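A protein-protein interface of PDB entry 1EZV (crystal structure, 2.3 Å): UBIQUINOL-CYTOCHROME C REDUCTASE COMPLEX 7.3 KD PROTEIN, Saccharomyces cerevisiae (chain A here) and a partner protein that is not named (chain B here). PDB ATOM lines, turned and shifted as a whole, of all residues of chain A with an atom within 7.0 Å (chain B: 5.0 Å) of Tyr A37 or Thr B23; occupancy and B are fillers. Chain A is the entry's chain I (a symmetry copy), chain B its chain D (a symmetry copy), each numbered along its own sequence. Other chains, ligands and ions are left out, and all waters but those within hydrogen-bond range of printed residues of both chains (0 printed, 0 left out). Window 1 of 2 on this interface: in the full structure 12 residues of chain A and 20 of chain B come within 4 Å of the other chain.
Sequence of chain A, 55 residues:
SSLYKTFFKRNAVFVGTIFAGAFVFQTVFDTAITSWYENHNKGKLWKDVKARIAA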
ATOM      1  N   THR A  31      -2.659 -12.448  -1.177  1.00  0.00           N
ATOM      2  CA  THR A  31      -2.022 -12.135  -2.455  1.00  0.00           C
ATOM      3  C   THR A  31      -2.741 -12.847  -3.599  1.00  0.00           C
ATOM      4  O   THR A  31      -3.074 -12.226  -4.607  1.00  0.00           O
ATOM      5  CB  THR A  31      -0.514 -12.527  -2.457  1.00  0.00           C
ATOM      6  OG1 THR A  31       0.168 -11.833  -1.403  1.00  0.00           O
ATOM      7  CG2 THR A  31       0.135 -12.150  -3.786  1.00  0.00           C
ATOM      8  N   ALA A  32      -3.085 -14.113  -3.383  1.00  0.00           N
ATOM      9  CA  ALA A  32      -3.837 -14.884  -4.372  1.00  0.00           C
ATOM     10  C   ALA A  32      -5.172 -14.225  -4.744  1.00  0.00           C
ATOM     11  O   ALA A  32      -5.539 -14.185  -5.922  1.00  0.00           O
ATOM     12  CB  ALA A  32      -4.075 -16.303  -3.860  1.00  0.00           C
ATOM     13  N   ILE A  33      -5.865 -13.675  -3.744  1.00  0.00           N
ATOM     14  CA  ILE A  33      -7.181 -13.069  -3.936  1.00  0.00           C
ATOM     15  C   ILE A  33      -7.064 -11.688  -4.573  1.00  0.00           C
ATOM     16  O   ILE A  33      -7.793 -11.377  -5.516  1.00  0.00           O
ATOM     17  CB  ILE A  33      -7.955 -12.947  -2.582  1.00  0.00           C
ATOM     18  CG1 ILE A  33      -8.266 -14.338  -2.028  1.00  0.00           C
ATOM     19  CG2 ILE A  33      -9.258 -12.163  -2.765  1.00  0.00           C
ATOM     20  CD1 ILE A  33      -9.090 -15.191  -2.957  1.00  0.00           C
ATOM     21  N   THR A  34      -6.159 -10.859  -4.060  1.00  0.00           N
ATOM     22  CA  THR A  34      -5.927  -9.544  -4.651  1.00  0.00           C
ATOM     23  C   THR A  34      -5.533  -9.666  -6.125  1.00  0.00           C
ATOM     24  O   THR A  34      -6.000  -8.893  -6.968  1.00  0.00           O
ATOM     25  CB  THR A  34      -4.815  -8.775  -3.918  1.00  0.00           C
ATOM     26  OG1 THR A  34      -5.194  -8.558  -2.553  1.00  0.00           O
ATOM     27  CG2 THR A  34      -4.567  -7.428  -4.595  1.00  0.00           C
ATOM     28  N   SER A  35      -4.711 -10.668  -6.436  1.00  0.00           N
ATOM     29  CA  SER A  35      -4.265 -10.896  -7.807  1.00  0.00           C
ATOM     30  C   SER A  35      -5.425 -11.231  -8.725  1.00  0.00           C
ATOM     31  O   SER A  35      -5.627 -10.569  -9.747  1.00  0.00           O
ATOM     32  CB  SER A  35      -3.228 -12.020  -7.862  1.00  0.00           C
ATOM     33  OG  SER A  35      -1.972 -11.544  -7.419  1.00  0.00           O
ATOM     34  N   TRP A  36      -6.202 -12.239  -8.341  1.00  0.00           N
ATOM     35  CA  TRP A  36      -7.383 -12.627  -9.102  1.00  0.00           C
ATOM     36  C   TRP A  36      -8.331 -11.437  -9.270  1.00  0.00           C
ATOM     37  O   TRP A  36      -8.767 -11.138 -10.380  1.00  0.00           O
ATOM     38  CB  TRP A  36      -8.102 -13.784  -8.405  1.00  0.00           C
ATOM     39  CG  TRP A  36      -9.262 -14.316  -9.180  1.00  0.00           C
ATOM     40  CD1 TRP A  36      -9.230 -15.301 -10.123  1.00  0.00           C
ATOM     41  CD2 TRP A  36     -10.610 -13.820  -9.163  1.00  0.00           C
ATOM     42  NE1 TRP A  36     -10.465 -15.433 -10.715  1.00  0.00           N
ATOM     43  CE2 TRP A  36     -11.331 -14.536 -10.145  1.00  0.00           C
ATOM     44  CE3 TRP A  36     -11.274 -12.835  -8.416  1.00  0.00           C
ATOM     45  CZ2 TRP A  36     -12.685 -14.297 -10.408  1.00  0.00           C
ATOM     46  CZ3 TRP A  36     -12.618 -12.594  -8.675  1.00  0.00           C
ATOM     47  CH2 TRP A  36     -13.310 -13.325  -9.664  1.00  0.00           C
ATOM     48  N   TYR A  37      -8.541 -10.694  -8.186  1.00  0.00           N
ATOM     49  CA  TYR A  37      -9.510  -9.601  -8.164  1.00  0.00           C
ATOM     50  C   TYR A  37      -9.104  -8.468  -9.103  1.00  0.00           C
ATOM     51  O   TYR A  37      -9.916  -8.007  -9.909  1.00  0.00           O
ATOM     52  CB  TYR A  37      -9.668  -9.072  -6.731  1.00  0.00           C
ATOM     53  CG  TYR A  37     -10.817  -8.108  -6.529  1.00  0.00           C
ATOM     54  CD1 TYR A  37     -12.144  -8.556  -6.543  1.00  0.00           C
ATOM     55  CD2 TYR A  37     -10.577  -6.765  -6.228  1.00  0.00           C
ATOM     56  CE1 TYR A  37     -13.202  -7.689  -6.261  1.00  0.00           C
ATOM     57  CE2 TYR A  37     -11.624  -5.893  -5.938  1.00  0.00           C
ATOM     58  CZ  TYR A  37     -12.932  -6.360  -5.962  1.00  0.00           C
ATOM     59  OH  TYR A  37     -13.961  -5.483  -5.733  1.00  0.00           O
ATOM     60  N   GLU A  38      -7.854  -8.024  -8.996  1.00  0.00           N
ATOM     61  CA  GLU A  38      -7.351  -6.937  -9.837  1.00  0.00           C
ATOM     62  C   GLU A  38      -7.291  -7.330 -11.316  1.00  0.00           C
ATOM     63  O   GLU A  38      -7.522  -6.499 -12.198  1.00  0.00           O
ATOM     64  CB  GLU A  38      -5.963  -6.502  -9.368  1.00  0.00           C
ATOM     65  CG  GLU A  38      -5.964  -5.745  -8.063  1.00  0.00           C
ATOM     66  CD  GLU A  38      -4.655  -5.024  -7.804  1.00  0.00           C
ATOM     67  OE1 GLU A  38      -4.699  -3.942  -7.178  1.00  0.00           O
ATOM     68  OE2 GLU A  38      -3.584  -5.542  -8.204  1.00  0.00           O
ATOM     69  N   ASN A  39      -6.992  -8.601 -11.574  1.00  0.00           N
ATOM     70  CA  ASN A  39      -6.974  -9.142 -12.929  1.00  0.00           C
ATOM     71  C   ASN A  39      -8.384  -9.197 -13.518  1.00  0.00           C
ATOM     72  O   ASN A  39      -8.619  -8.720 -14.630  1.00  0.00           O
ATOM     73  CB  ASN A  39      -6.355 -10.547 -12.924  1.00  0.00           C
ATOM     74  CG  ASN A  39      -6.295 -11.165 -14.311  1.00  0.00           C
ATOM     75  OD1 ASN A  39      -5.549 -10.703 -15.178  1.00  0.00           O
ATOM     76  ND2 ASN A  39      -7.103 -12.198 -14.536  1.00  0.00           N
ATOM     77  N   HIS A  40      -9.319  -9.773 -12.766  1.00  0.00           N
ATOM     78  CA  HIS A  40     -10.720  -9.833 -13.176  1.00  0.00           C
ATOM     79  C   HIS A  40     -11.276  -8.452 -13.523  1.00  0.00           C
ATOM     80  O   HIS A  40     -12.151  -8.331 -14.374  1.00  0.00           O
ATOM     81  CB  HIS A  40     -11.572 -10.481 -12.069  1.00  0.00           C
ATOM     82  CG  HIS A  40     -13.026 -10.595 -12.413  1.00  0.00           C
ATOM     83  ND1 HIS A  40     -13.550 -11.684 -13.079  1.00  0.00           N
ATOM     84  CD2 HIS A  40     -14.049  -9.720 -12.262  1.00  0.00           C
ATOM     85  CE1 HIS A  40     -14.827 -11.470 -13.332  1.00  0.00           C
ATOM     86  NE2 HIS A  40     -15.154 -10.283 -12.849  1.00  0.00           N
ATOM     87  N   ASN A  41     -10.752  -7.414 -12.878  1.00  0.00           N
ATOM     88  CA  ASN A  41     -11.220  -6.050 -13.110  1.00  0.00           C
ATOM     89  C   ASN A  41     -10.272  -5.183 -13.943  1.00  0.00           C
ATOM     90  O   ASN A  41     -10.349  -3.950 -13.909  1.00  0.00           O
ATOM     91  CB  ASN A  41     -11.512  -5.367 -11.772  1.00  0.00           C
ATOM     92  CG  ASN A  41     -12.869  -5.740 -11.222  1.00  0.00           C
ATOM     93  OD1 ASN A  41     -13.880  -5.143 -11.592  1.00  0.00           O
ATOM     94  ND2 ASN A  41     -12.909  -6.777 -10.390  1.00  0.00           N
ATOM     95  N   LYS A  42      -9.446  -5.837 -14.756  1.00  0.00           N
ATOM     96  CA  LYS A  42      -8.512  -5.159 -15.650  1.00  0.00           C
ATOM     97  C   LYS A  42      -9.245  -4.200 -16.590  1.00  0.00           C
ATOM     98  O   LYS A  42     -10.289  -4.537 -17.148  1.00  0.00           O
ATOM     99  CB  LYS A  42      -7.733  -6.194 -16.468  1.00  0.00           C
ATOM    100  CG  LYS A  42      -6.355  -5.732 -16.913  1.00  0.00           C
ATOM    101  CD  LYS A  42      -5.768  -6.682 -17.952  1.00  0.00           C
ATOM    102  CE  LYS A  42      -5.311  -8.000 -17.325  1.00  0.00           C
ATOM    103  NZ  LYS A  42      -4.205  -7.805 -16.336  1.00  0.00           N
ATOM    104  N   LYS A  44     -10.690  -1.364 -15.539  1.00  0.00           N
ATOM    105  CA  LYS A  44     -11.558  -0.521 -14.722  1.00  0.00           C
ATOM    106  C   LYS A  44     -10.824   0.160 -13.579  1.00  0.00           C
ATOM    107  O   LYS A  44     -11.249   1.216 -13.110  1.00  0.00           O
ATOM    108  CB  LYS A  44     -12.711  -1.353 -14.166  1.00  0.00           C
ATOM    109  CG  LYS A  44     -13.759  -1.723 -15.197  1.00  0.00           C
ATOM    110  CD  LYS A  44     -14.359  -3.092 -14.922  1.00  0.00           C
ATOM    111  CE  LYS A  44     -15.259  -3.073 -13.707  1.00  0.00           C
ATOM    112  NZ  LYS A  44     -15.762  -4.434 -13.383  1.00  0.00           N
ATOM    113  N   LEU A  45      -9.712  -0.435 -13.152  1.00  0.00           N
ATOM    114  CA  LEU A  45      -8.928   0.067 -12.020  1.00  0.00           C
ATOM    115  C   LEU A  45      -8.310   1.439 -12.270  1.00  0.00           C
ATOM    116  O   LEU A  45      -8.108   1.843 -13.417  1.00  0.00           O
ATOM    117  CB  LEU A  45      -7.811  -0.919 -11.674  1.00  0.00           C
ATOM    118  CG  LEU A  45      -8.036  -2.023 -10.639  1.00  0.00           C
ATOM    119  CD1 LEU A  45      -9.513  -2.143 -10.265  1.00  0.00           C
ATOM    120  CD2 LEU A  45      -7.500  -3.333 -11.201  1.00  0.00           C
ATOM    121  N   SER B  16     -21.419  -1.673 -14.857  1.00  0.00           N
ATOM    122  CA  SER B  16     -20.230  -2.511 -14.863  1.00  0.00           C
ATOM    123  C   SER B  16     -19.777  -2.853 -13.436  1.00  0.00           C
ATOM    124  O   SER B  16     -19.076  -3.846 -13.225  1.00  0.00           O
ATOM    125  CB  SER B  16     -19.098  -1.839 -15.658  1.00  0.00           C
ATOM    126  OG  SER B  16     -18.872  -0.501 -15.239  1.00  0.00           O
ATOM    127  N   HIS B  17     -20.263  -2.089 -12.456  1.00  0.00           N
ATOM    128  CA  HIS B  17     -20.025  -2.409 -11.045  1.00  0.00           C
ATOM    129  C   HIS B  17     -21.061  -3.341 -10.391  1.00  0.00           C
ATOM    130  O   HIS B  17     -20.901  -3.717  -9.229  1.00  0.00           O
ATOM    131  CB  HIS B  17     -19.883  -1.129 -10.217  1.00  0.00           C
ATOM    132  CG  HIS B  17     -20.959  -0.116 -10.457  1.00  0.00           C
ATOM    133  ND1 HIS B  17     -22.026   0.048  -9.600  1.00  0.00           N
ATOM    134  CD2 HIS B  17     -21.046   0.894 -11.357  1.00  0.00           C
ATOM    135  CE1 HIS B  17     -22.714   1.120  -9.950  1.00  0.00           C
ATOM    136  NE2 HIS B  17     -22.140   1.652 -11.013  1.00  0.00           N
ATOM    137  N   PRO B  20     -20.884  -9.422  -7.841  1.00  0.00           N
ATOM    138  CA  PRO B  20     -20.089  -9.547  -6.612  1.00  0.00           C
ATOM    139  C   PRO B  20     -18.588  -9.334  -6.806  1.00  0.00           C
ATOM    140  O   PRO B  20     -17.910  -8.821  -5.906  1.00  0.00           O
ATOM    141  CB  PRO B  20     -20.411 -10.961  -6.108  1.00  0.00           C
ATOM    142  CG  PRO B  20     -21.007 -11.669  -7.290  1.00  0.00           C
ATOM    143  CD  PRO B  20     -21.707 -10.618  -8.086  1.00  0.00           C
ATOM    144  N   PHE B  21     -18.098  -9.623  -8.011  1.00  0.00           N
ATOM    145  CA  PHE B  21     -16.668  -9.541  -8.298  1.00  0.00           C
ATOM    146  C   PHE B  21     -16.251  -8.238  -8.976  1.00  0.00           C
ATOM    147  O   PHE B  21     -15.071  -8.033  -9.230  1.00  0.00           O
ATOM    148  CB  PHE B  21     -16.225 -10.720  -9.168  1.00  0.00           C
ATOM    149  CG  PHE B  21     -16.677 -12.063  -8.659  1.00  0.00           C
ATOM    150  CD1 PHE B  21     -17.402 -12.921  -9.479  1.00  0.00           C
ATOM    151  CD2 PHE B  21     -16.368 -12.476  -7.371  1.00  0.00           C
ATOM    152  CE1 PHE B  21     -17.815 -14.173  -9.021  1.00  0.00           C
ATOM    153  CE2 PHE B  21     -16.776 -13.725  -6.904  1.00  0.00           C
ATOM    154  CZ  PHE B  21     -17.501 -14.574  -7.728  1.00  0.00           C
ATOM    155  N   GLU B  22     -17.189  -7.311  -9.151  1.00  0.00           N
ATOM    156  CA  GLU B  22     -16.949  -6.135  -9.988  1.00  0.00           C
ATOM    157  C   GLU B  22     -16.620  -4.853  -9.236  1.00  0.00           C
ATOM    158  O   GLU B  22     -17.435  -4.357  -8.459  1.00  0.00           O
ATOM    159  CB  GLU B  22     -18.157  -5.882 -10.891  1.00  0.00           C
ATOM    160  CG  GLU B  22     -18.630  -7.107 -11.662  1.00  0.00           C
ATOM    161  CD  GLU B  22     -17.538  -7.720 -12.518  1.00  0.00           C
ATOM    162  OE1 GLU B  22     -17.456  -8.965 -12.574  1.00  0.00           O
ATOM    163  OE2 GLU B  22     -16.760  -6.959 -13.130  1.00  0.00           O
ATOM    164  N   THR B  23     -15.493  -4.238  -9.587  1.00  0.00           N
ATOM    165  CA  THR B  23     -15.141  -2.917  -9.069  1.00  0.00           C
ATOM    166  C   THR B  23     -15.882  -1.834  -9.845  1.00  0.00           C
ATOM    167  O   THR B  23     -16.462  -2.105 -10.893  1.00  0.00           O
ATOM    168  CB  THR B  23     -13.626  -2.634  -9.188  1.00  0.00           C
ATOM    169  OG1 THR B  23     -13.243  -2.607 -10.573  1.00  0.00           O
ATOM    170  CG2 THR B  23     -12.827  -3.699  -8.457  1.00  0.00           C
ATOM    171  N   PHE B  24     -15.839  -0.605  -9.346  1.00  0.00           N
ATOM    172  CA  PHE B  24     -16.236   0.541 -10.153  1.00  0.00           C
ATOM    173  C   PHE B  24     -15.343   0.623 -11.395  1.00  0.00           C
ATOM    174  O   PHE B  24     -14.202   0.141 -11.391  1.00  0.00           O
ATOM    175  CB  PHE B  24     -16.080   1.845  -9.366  1.00  0.00           C
ATOM    176  CG  PHE B  24     -17.139   2.070  -8.330  1.00  0.00           C
ATOM    177  CD1 PHE B  24     -16.794   2.559  -7.070  1.00  0.00           C
ATOM    178  CD2 PHE B  24     -18.482   1.897  -8.633  1.00  0.00           C
ATOM    179  CE1 PHE B  24     -17.774   2.884  -6.138  1.00  0.00           C
ATOM    180  CE2 PHE B  24     -19.471   2.216  -7.701  1.00  0.00           C
ATOM    181  CZ  PHE B  24     -19.114   2.712  -6.457  1.00  0.00           C
ATOM    182  N   ASP B  25     -15.862   1.258 -12.439  1.00  0.00           N
ATOM    183  CA  ASP B  25     -15.034   1.720 -13.542  1.00  0.00           C
ATOM    184  C   ASP B  25     -14.534   3.115 -13.187  1.00  0.00           C
ATOM    185  O   ASP B  25     -15.302   4.077 -13.189  1.00  0.00           O
ATOM    186  CB  ASP B  25     -15.856   1.772 -14.829  1.00  0.00           C
ATOM    187  CG  ASP B  25     -15.002   2.005 -16.063  1.00  0.00           C
ATOM    188  OD1 ASP B  25     -14.969   1.106 -16.927  1.00  0.00           O
ATOM    189  OD2 ASP B  25     -14.407   3.096 -16.197  1.00  0.00           O
ATOM    190  N   HIS B 202     -16.673   0.715  -1.719  1.00  0.00           N
ATOM    191  CA  HIS B 202     -17.164  -0.300  -2.659  1.00  0.00           C
ATOM    192  C   HIS B 202     -16.148  -1.358  -3.125  1.00  0.00           C
ATOM    193  O   HIS B 202     -16.353  -2.556  -2.905  1.00  0.00           O
ATOM    194  CB  HIS B 202     -17.787   0.409  -3.870  1.00  0.00           C
ATOM    195  CG  HIS B 202     -18.356  -0.513  -4.905  1.00  0.00           C
ATOM    196  ND1 HIS B 202     -17.656  -0.890  -6.032  1.00  0.00           N
ATOM    197  CD2 HIS B 202     -19.571  -1.100  -5.004  1.00  0.00           C
ATOM    198  CE1 HIS B 202     -18.408  -1.685  -6.772  1.00  0.00           C
ATOM    199  NE2 HIS B 202     -19.576  -1.829  -6.173  1.00  0.00           N
ATOM    200  N   ASP B 203     -15.058  -0.924  -3.758  1.00  0.00           N
ATOM    201  CA  ASP B 203     -14.128  -1.869  -4.393  1.00  0.00           C
ATOM    202  C   ASP B 203     -13.421  -2.736  -3.363  1.00  0.00           C
ATOM    203  O   ASP B 203     -13.306  -3.950  -3.524  1.00  0.00           O
ATOM    204  CB  ASP B 203     -13.078  -1.119  -5.221  1.00  0.00           C
ATOM    205  CG  ASP B 203     -13.680  -0.366  -6.390  1.00  0.00           C
ATOM    206  OD1 ASP B 203     -14.850  -0.618  -6.750  1.00  0.00           O
ATOM    207  OD2 ASP B 203     -12.982   0.500  -6.946  1.00  0.00           O
ATOM    208  N   GLU B 204     -12.965  -2.087  -2.299  1.00  0.00           N
ATOM    209  CA  GLU B 204     -12.324  -2.757  -1.180  1.00  0.00           C
ATOM    210  C   GLU B 204     -13.288  -3.648  -0.395  1.00  0.00           C
ATOM    211  O   GLU B 204     -12.929  -4.769  -0.024  1.00  0.00           O
ATOM    212  CB  GLU B 204     -11.681  -1.709  -0.265  1.00  0.00           C
ATOM    213  CG  GLU B 204     -10.963  -2.265   0.945  1.00  0.00           C
ATOM    214  CD  GLU B 204      -9.786  -3.199   0.618  1.00  0.00           C
ATOM    215  OE1 GLU B 204      -9.102  -3.617   1.578  1.00  0.00           O
ATOM    216  OE2 GLU B 204      -9.553  -3.544  -0.565  1.00  0.00           O
ATOM    217  N   LYS B 206     -15.875  -5.327  -1.451  1.00  0.00           N
ATOM    218  CA  LYS B 206     -16.168  -6.556  -2.183  1.00  0.00           C
ATOM    219  C   LYS B 206     -14.977  -7.506  -2.223  1.00  0.00           C
ATOM    220  O   LYS B 206     -15.141  -8.717  -2.361  1.00  0.00           O
ATOM    221  CB  LYS B 206     -16.596  -6.234  -3.609  1.00  0.00           C
ATOM    222  CG  LYS B 206     -17.964  -5.593  -3.727  1.00  0.00           C
ATOM    223  CD  LYS B 206     -18.567  -5.925  -5.067  1.00  0.00           C
ATOM    224  CE  LYS B 206     -19.539  -4.863  -5.493  1.00  0.00           C
ATOM    225  NZ  LYS B 206     -20.009  -5.109  -6.875  1.00  0.00           N
ATOM    226  N   ARG B 207     -13.778  -6.938  -2.181  1.00  0.00           N
ATOM    227  CA  ARG B 207     -12.551  -7.724  -2.130  1.00  0.00           C
ATOM    228  C   ARG B 207     -12.447  -8.452  -0.785  1.00  0.00           C
ATOM    229  O   ARG B 207     -12.160  -9.651  -0.739  1.00  0.00           O
ATOM    230  CB  ARG B 207     -11.352  -6.794  -2.327  1.00  0.00           C
ATOM    231  CG  ARG B 207     -10.057  -7.487  -2.671  1.00  0.00           C
ATOM    232  CD  ARG B 207      -8.875  -6.594  -2.322  1.00  0.00           C
ATOM    233  NE  ARG B 207      -7.999  -7.284  -1.388  1.00  0.00           N
ATOM    234  CZ  ARG B 207      -7.715  -6.861  -0.163  1.00  0.00           C
ATOM    235  NH1 ARG B 207      -7.053  -7.657   0.661  1.00  0.00           N
ATOM    236  NH2 ARG B 207      -7.985  -5.619   0.202  1.00  0.00           N
ATOM    237  N   LEU B 210     -15.026 -11.320  -0.586  1.00  0.00           N
ATOM    238  CA  LEU B 210     -14.565 -12.506  -1.298  1.00  0.00           C
ATOM    239  C   LEU B 210     -13.712 -13.411  -0.403  1.00  0.00           C
ATOM    240  O   LEU B 210     -13.966 -14.613  -0.313  1.00  0.00           O
ATOM    241  CB  LEU B 210     -13.776 -12.080  -2.543  1.00  0.00           C
ATOM    242  CG  LEU B 210     -13.212 -13.170  -3.468  1.00  0.00           C
ATOM    243  CD1 LEU B 210     -14.299 -14.171  -3.867  1.00  0.00           C
ATOM    244  CD2 LEU B 210     -12.610 -12.503  -4.702  1.00  0.00           C
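OE1 of Glu B22 is in hydrogen-bond range of NE2 of His A40, at 2.7 Å.
The side-chain amide oxygen (OD1) of Asn A41 is in hydrogen-bond range of the backbone NH (N) of Thr B23 (2.7 Å).
The backbone carbonyl oxygen (O) of Asp B203 is in hydrogen-bond range of the side-chain hydroxyl (OH) of Tyr A37, at 2.8 Å.
The backbone carbonyl oxygen of Ser B16 is in hydrogen-bond range of the side-chain amino group of Lys A44.
The side-chain amino group (NZ) of Lys A44 lies close to the backbone carbonyl oxygen (O) of Thr B23, at 3.5 Å.
NE of Arg B207 lies within hydrogen-bond range of OG1 of Thr A34, 3.3 Å away.
The backbone carbonyl oxygen (O) of Phe B21 sits at hydrogen-bond distance from the side-chain amide nitrogen (ND2) of Asn A41 (2.8 Å).
The side-chain carboxylate (OE2) of Glu B22 lies within salt-bridge range of the side-chain amino group (NZ) of Lys A44, at 2.7 Å.
Thr A31 touches none of the printed residues of chain B.
Of the printed residues of chain B, Ile A33 touches Leu B210.
Printed residues of chain B within 4 Å of Tyr A37: Phe B21 (3.5 Å), Thr B23 (3.4 Å), Asp B203 (2.8 Å), Lys B206 (3.5 Å) and Arg B207 (3.7 Å).
Of the printed residues of chain B, Lys A44 touches Ser B16, Glu B22, Thr B23, Phe B24 and Asp B25.
Thr B23 touches four residues of chain A.
Glu B204 touches none of the printed residues of chain A.
Of the printed residues of chain A, Lys B206 touches Tyr A37 (3.5 Å).
The nearest residue of chain A that does not touch Thr B23 is His A40 (6.3 Å).
Among the printed residues, pairs that only touch across the chains: Tyr A37 with Thr B23, Tyr A37 with Lys B206, Lys A44 with Phe B24, Tyr A37 with Phe B21, Lys A44 with Asp B25, Asn A41 with Glu B22, His A40 with Phe B21, Tyr A37 with Arg B207, Trp A36 with Phe B21, Leu A45 with Thr B23, Ile A33 with Leu B210 and Trp A36 with Leu B210.
Printed residues of chain A that touch a printed residue of chain B: Ile A33, Thr A34, Trp A36, Tyr A37, His A40, Asn A41, Lys A44 and Leu A45.
Of the 14 printed residues of chain B, 10 touch a printed residue of chain A.
Among the printed residues, 20 pairs touch across the chains.
Among the printed residues, Asp or Glu carboxylates within 4 Å of a Lys or Arg side-chain nitrogen of the other chain: Lys A44 with Glu B22 (2.7 Å).
A ring nitrogen (NE2) of His B202 lies close to the side-chain amino group of Lys B206 (3.4 Å).
The side-chain amino group of Lys B206 lies within hydrogen-bond range of the backbone carbonyl oxygen of Glu B22 (3.1 Å).
OD1 of Asn A41 is in hydrogen-bond range of NZ of Lys A44 (2.7 Å).
The side-chain carboxylate (OD1) of Asp B203 lies within hydrogen-bond range of the backbone NH (N) of Phe B24, at 2.8 Å.
OD1 of Asp B203 sits at hydrogen-bond distance from ND1 of His B202, at 2.9 Å.
The side-chain carboxylate of Glu B204 lies within salt-bridge range of the guanidinium group of Arg B207, at 2.7 Å.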
